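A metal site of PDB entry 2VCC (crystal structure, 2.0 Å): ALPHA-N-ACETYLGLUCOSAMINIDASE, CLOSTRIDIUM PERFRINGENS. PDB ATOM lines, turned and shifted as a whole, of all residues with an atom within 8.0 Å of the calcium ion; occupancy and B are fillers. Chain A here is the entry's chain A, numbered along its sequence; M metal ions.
O of Asp 28 sits close to OG1 of Thr 31 (3.4 Å).
OG of Ser 30 sits at hydrogen-bond distance from OD1 of Asp 28 (2.7 Å).
The backbone NH of Ala 123 sits at hydrogen-bond distance from the backbone carbonyl oxygen of Phe 58 (2.6 Å).
The side-chain carboxylate (OE1) of Glu 124 lies within hydrogen-bond range of the backbone NH (N) of Gly 27, at 2.9 Å.
The backbone NH of Phe 58 sits at hydrogen-bond distance from the backbone carbonyl oxygen of Glu 124, at 2.9 Å.
Of the 19 residues printed, 6 come within 4 Å of the calcium ion.
The nearest printed residue that does not touch the calcium ion is Tyr 32 (4.2 Å).
The calcium ion is bound by the backbone carbonyl oxygen (O) of Leu 23 (2.3 Å), the backbone carbonyl oxygen (O) of Asp 28 (2.3 Å), the backbone carbonyl oxygen (O) of Ala 123 (2.3 Å), the backbone carbonyl oxygen (O) of Thr 31 (2.3 Å), the side-chain carboxylate (OE2) of Glu 124 (2.4 Å) and the side-chain carboxylate (OD1) of Asp 26 (2.4 Å).
The calcium ion has six donor atoms within binding distance.
Slightly farther from the calcium ion lies OG1 of Thr 31 (2.9 Å).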
ATOM      1  N   THR A  20       6.653  -2.664 -24.981  1.00  0.00           N
ATOM      2  CA  THR A  20       8.001  -3.203 -24.928  1.00  0.00           C
ATOM      3  C   THR A  20       8.051  -4.735 -24.901  1.00  0.00           C
ATOM      4  O   THR A  20       7.034  -5.391 -24.655  1.00  0.00           O
ATOM      5  CB  THR A  20       8.767  -2.647 -23.709  1.00  0.00           C
ATOM      6  OG1 THR A  20       7.958  -2.778 -22.532  1.00  0.00           O
ATOM      7  CG2 THR A  20       9.109  -1.173 -23.914  1.00  0.00           C
ATOM      8  N   ALA A  21       9.233  -5.288 -25.157  1.00  0.00           N
ATOM      9  CA  ALA A  21       9.435  -6.749 -25.223  1.00  0.00           C
ATOM     10  C   ALA A  21       9.018  -7.536 -23.971  1.00  0.00           C
ATOM     11  O   ALA A  21       8.368  -8.584 -24.088  1.00  0.00           O
ATOM     12  CB  ALA A  21      10.888  -7.066 -25.582  1.00  0.00           C
ATOM     13  N   ASP A  22       9.380  -7.027 -22.796  1.00  0.00           N
ATOM     14  CA  ASP A  22       9.031  -7.637 -21.513  1.00  0.00           C
ATOM     15  C   ASP A  22       7.522  -7.826 -21.331  1.00  0.00           C
ATOM     16  O   ASP A  22       7.097  -8.692 -20.569  1.00  0.00           O
ATOM     17  CB  ASP A  22       9.610  -6.828 -20.354  1.00  0.00           C
ATOM     18  CG  ASP A  22       9.057  -5.417 -20.298  1.00  0.00           C
ATOM     19  OD1 ASP A  22       8.533  -5.017 -19.232  1.00  0.00           O
ATOM     20  OD2 ASP A  22       9.142  -4.708 -21.319  1.00  0.00           O
ATOM     21  N   LEU A  23       6.721  -7.047 -22.049  1.00  0.00           N
ATOM     22  CA  LEU A  23       5.260  -7.173 -21.977  1.00  0.00           C
ATOM     23  C   LEU A  23       4.718  -8.430 -22.664  1.00  0.00           C
ATOM     24  O   LEU A  23       3.553  -8.796 -22.486  1.00  0.00           O
ATOM     25  CB  LEU A  23       4.561  -5.903 -22.466  1.00  0.00           C
ATOM     26  CG  LEU A  23       4.868  -4.610 -21.701  1.00  0.00           C
ATOM     27  CD1 LEU A  23       3.992  -3.472 -22.192  1.00  0.00           C
ATOM     28  CD2 LEU A  23       4.766  -4.754 -20.167  1.00  0.00           C
ATOM     29  N   ALA A  24       5.570  -9.101 -23.428  1.00  0.00           N
ATOM     30  CA  ALA A  24       5.216 -10.397 -24.024  1.00  0.00           C
ATOM     31  C   ALA A  24       5.275 -11.529 -23.012  1.00  0.00           C
ATOM     32  O   ALA A  24       4.729 -12.615 -23.257  1.00  0.00           O
ATOM     33  CB  ALA A  24       6.128 -10.694 -25.215  1.00  0.00           C
ATOM     34  N   ILE A  25       5.940 -11.301 -21.881  1.00  0.00           N
ATOM     35  CA  ILE A  25       6.161 -12.348 -20.874  1.00  0.00           C
ATOM     36  C   ILE A  25       5.809 -11.926 -19.442  1.00  0.00           C
ATOM     37  O   ILE A  25       6.450 -12.364 -18.479  1.00  0.00           O
ATOM     38  CB  ILE A  25       7.609 -12.918 -20.927  1.00  0.00           C
ATOM     39  CG1 ILE A  25       8.656 -11.811 -20.766  1.00  0.00           C
ATOM     40  CG2 ILE A  25       7.839 -13.744 -22.189  1.00  0.00           C
ATOM     41  CD1 ILE A  25       9.963 -12.277 -20.161  1.00  0.00           C
ATOM     42  N   ASP A  26       4.770 -11.105 -19.279  1.00  0.00           N
ATOM     43  CA  ASP A  26       4.456 -10.539 -17.951  1.00  0.00           C
ATOM     44  C   ASP A  26       3.228 -11.151 -17.264  1.00  0.00           C
ATOM     45  O   ASP A  26       2.798 -10.667 -16.223  1.00  0.00           O
ATOM     46  CB  ASP A  26       4.373  -9.008 -18.006  1.00  0.00           C
ATOM     47  CG  ASP A  26       3.183  -8.497 -18.802  1.00  0.00           C
ATOM     48  OD1 ASP A  26       2.563  -9.279 -19.553  1.00  0.00           O
ATOM     49  OD2 ASP A  26       2.878  -7.286 -18.708  1.00  0.00           O
ATOM     50  N   GLY A  27       2.695 -12.226 -17.839  1.00  0.00           N
ATOM     51  CA  GLY A  27       1.544 -12.948 -17.272  1.00  0.00           C
ATOM     52  C   GLY A  27       0.218 -12.264 -17.489  1.00  0.00           C
ATOM     53  O   GLY A  27      -0.813 -12.747 -17.036  1.00  0.00           O
ATOM     54  N   ASP A  28       0.243 -11.136 -18.208  1.00  0.00           N
ATOM     55  CA  ASP A  28      -0.897 -10.248 -18.381  1.00  0.00           C
ATOM     56  C   ASP A  28      -1.282 -10.215 -19.857  1.00  0.00           C
ATOM     57  O   ASP A  28      -0.456  -9.870 -20.700  1.00  0.00           O
ATOM     58  CB  ASP A  28      -0.516  -8.859 -17.874  1.00  0.00           C
ATOM     59  CG  ASP A  28      -1.708  -7.917 -17.750  1.00  0.00           C
ATOM     60  OD1 ASP A  28      -2.822  -8.250 -18.205  1.00  0.00           O
ATOM     61  OD2 ASP A  28      -1.515  -6.813 -17.190  1.00  0.00           O
ATOM     62  N   LEU A  29      -2.525 -10.570 -20.158  1.00  0.00           N
ATOM     63  CA  LEU A  29      -3.007 -10.671 -21.524  1.00  0.00           C
ATOM     64  C   LEU A  29      -3.338  -9.313 -22.123  1.00  0.00           C
ATOM     65  O   LEU A  29      -3.457  -9.169 -23.350  1.00  0.00           O
ATOM     66  CB  LEU A  29      -4.247 -11.578 -21.583  1.00  0.00           C
ATOM     67  CG  LEU A  29      -4.130 -13.035 -22.048  1.00  0.00           C
ATOM     68  CD1 LEU A  29      -2.754 -13.641 -21.859  1.00  0.00           C
ATOM     69  CD2 LEU A  29      -5.156 -13.858 -21.339  1.00  0.00           C
ATOM     70  N   SER A  30      -3.468  -8.310 -21.244  1.00  0.00           N
ATOM     71  CA  SER A  30      -3.891  -6.977 -21.639  1.00  0.00           C
ATOM     72  C   SER A  30      -2.718  -6.095 -22.058  1.00  0.00           C
ATOM     73  O   SER A  30      -2.917  -5.025 -22.632  1.00  0.00           O
ATOM     74  CB  SER A  30      -4.669  -6.303 -20.507  1.00  0.00           C
ATOM     75  OG  SER A  30      -3.811  -6.041 -19.407  1.00  0.00           O
ATOM     76  N   THR A  31      -1.501  -6.553 -21.752  1.00  0.00           N
ATOM     77  CA  THR A  31      -0.285  -5.850 -22.167  1.00  0.00           C
ATOM     78  C   THR A  31       0.447  -6.677 -23.235  1.00  0.00           C
ATOM     79  O   THR A  31       0.455  -7.909 -23.153  1.00  0.00           O
ATOM     80  CB  THR A  31       0.663  -5.577 -20.987  1.00  0.00           C
ATOM     81  OG1 THR A  31       1.121  -6.817 -20.432  1.00  0.00           O
ATOM     82  CG2 THR A  31      -0.027  -4.761 -19.892  1.00  0.00           C
ATOM     83  N   TYR A  32       1.068  -6.008 -24.192  1.00  0.00           N
ATOM     84  CA  TYR A  32       1.718  -6.697 -25.320  1.00  0.00           C
ATOM     85  C   TYR A  32       2.973  -5.998 -25.824  1.00  0.00           C
ATOM     86  O   TYR A  32       3.078  -4.777 -25.754  1.00  0.00           O
ATOM     87  CB  TYR A  32       0.716  -6.849 -26.459  1.00  0.00           C
ATOM     88  CG  TYR A  32       0.089  -5.549 -26.917  1.00  0.00           C
ATOM     89  CD1 TYR A  32      -1.131  -5.117 -26.392  1.00  0.00           C
ATOM     90  CD2 TYR A  32       0.709  -4.748 -27.884  1.00  0.00           C
ATOM     91  CE1 TYR A  32      -1.713  -3.915 -26.822  1.00  0.00           C
ATOM     92  CE2 TYR A  32       0.144  -3.569 -28.313  1.00  0.00           C
ATOM     93  CZ  TYR A  32      -1.067  -3.148 -27.787  1.00  0.00           C
ATOM     94  OH  TYR A  32      -1.626  -1.964 -28.221  1.00  0.00           O
ATOM     95  N   TRP A  33       3.931  -6.782 -26.326  1.00  0.00           N
ATOM     96  CA  TRP A  33       4.982  -6.262 -27.196  1.00  0.00           C
ATOM     97  C   TRP A  33       4.377  -5.987 -28.568  1.00  0.00           C
ATOM     98  O   TRP A  33       3.521  -6.729 -29.037  1.00  0.00           O
ATOM     99  CB  TRP A  33       6.144  -7.253 -27.311  1.00  0.00           C
ATOM    100  CG  TRP A  33       7.045  -6.984 -28.501  1.00  0.00           C
ATOM    101  CD1 TRP A  33       8.053  -6.056 -28.571  1.00  0.00           C
ATOM    102  CD2 TRP A  33       7.012  -7.627 -29.779  1.00  0.00           C
ATOM    103  NE1 TRP A  33       8.638  -6.087 -29.809  1.00  0.00           N
ATOM    104  CE2 TRP A  33       8.033  -7.045 -30.571  1.00  0.00           C
ATOM    105  CE3 TRP A  33       6.221  -8.654 -30.335  1.00  0.00           C
ATOM    106  CZ2 TRP A  33       8.278  -7.450 -31.899  1.00  0.00           C
ATOM    107  CZ3 TRP A  33       6.471  -9.055 -31.652  1.00  0.00           C
ATOM    108  CH2 TRP A  33       7.494  -8.451 -32.419  1.00  0.00           C
ATOM    109  N   PHE A  58      -0.407 -15.868 -27.356  1.00  0.00           N
ATOM    110  CA  PHE A  58      -1.557 -14.984 -27.368  1.00  0.00           C
ATOM    111  C   PHE A  58      -1.207 -13.703 -28.090  1.00  0.00           C
ATOM    112  O   PHE A  58      -0.127 -13.143 -27.899  1.00  0.00           O
ATOM    113  CB  PHE A  58      -1.987 -14.628 -25.932  1.00  0.00           C
ATOM    114  CG  PHE A  58      -2.531 -15.775 -25.155  1.00  0.00           C
ATOM    115  CD1 PHE A  58      -3.889 -16.042 -25.154  1.00  0.00           C
ATOM    116  CD2 PHE A  58      -1.675 -16.601 -24.426  1.00  0.00           C
ATOM    117  CE1 PHE A  58      -4.401 -17.108 -24.431  1.00  0.00           C
ATOM    118  CE2 PHE A  58      -2.180 -17.662 -23.708  1.00  0.00           C
ATOM    119  CZ  PHE A  58      -3.538 -17.921 -23.719  1.00  0.00           C
ATOM    120  N   ILE A 122       2.745  -9.835 -29.694  1.00  0.00           N
ATOM    121  CA  ILE A 122       2.565 -10.996 -28.831  1.00  0.00           C
ATOM    122  C   ILE A 122       2.087 -10.461 -27.469  1.00  0.00           C
ATOM    123  O   ILE A 122       2.784  -9.683 -26.832  1.00  0.00           O
ATOM    124  CB  ILE A 122       3.879 -11.810 -28.696  1.00  0.00           C
ATOM    125  CG1 ILE A 122       4.249 -12.460 -30.047  1.00  0.00           C
ATOM    126  CG2 ILE A 122       3.755 -12.905 -27.629  1.00  0.00           C
ATOM    127  CD1 ILE A 122       5.719 -12.700 -30.264  1.00  0.00           C
ATOM    128  N   ALA A 123       0.879 -10.851 -27.075  1.00  0.00           N
ATOM    129  CA  ALA A 123       0.328 -10.428 -25.786  1.00  0.00           C
ATOM    130  C   ALA A 123       0.925 -11.257 -24.650  1.00  0.00           C
ATOM    131  O   ALA A 123       1.260 -10.716 -23.600  1.00  0.00           O
ATOM    132  CB  ALA A 123      -1.189 -10.512 -25.773  1.00  0.00           C
ATOM    133  N   GLU A 124       1.025 -12.575 -24.860  1.00  0.00           N
ATOM    134  CA  GLU A 124       1.717 -13.472 -23.934  1.00  0.00           C
ATOM    135  C   GLU A 124       2.340 -14.655 -24.667  1.00  0.00           C
ATOM    136  O   GLU A 124       1.818 -15.111 -25.679  1.00  0.00           O
ATOM    137  CB  GLU A 124       0.767 -14.007 -22.856  1.00  0.00           C
ATOM    138  CG  GLU A 124       0.539 -13.087 -21.657  1.00  0.00           C
ATOM    139  CD  GLU A 124       1.808 -12.750 -20.918  1.00  0.00           C
ATOM    140  OE1 GLU A 124       2.450 -13.669 -20.364  1.00  0.00           O
ATOM    141  OE2 GLU A 124       2.155 -11.554 -20.869  1.00  0.00           O
ATOM    142  N   ILE A 125       3.464 -15.139 -24.140  1.00  0.00           N
ATOM    143  CA  ILE A 125       4.001 -16.423 -24.575  1.00  0.00           C
ATOM    144  C   ILE A 125       4.373 -17.291 -23.376  1.00  0.00           C
ATOM    145  O   ILE A 125       5.170 -16.890 -22.526  1.00  0.00           O
ATOM    146  CB  ILE A 125       5.185 -16.292 -25.577  1.00  0.00           C
ATOM    147  CG1 ILE A 125       5.726 -17.674 -25.942  1.00  0.00           C
ATOM    148  CG2 ILE A 125       6.266 -15.351 -25.030  1.00  0.00           C
ATOM    149  CD1 ILE A 125       6.803 -17.696 -26.985  1.00  0.00           C
HETATM  150 CA    CA M   1       1.506  -9.393 -21.732  1.00  0.00          CA
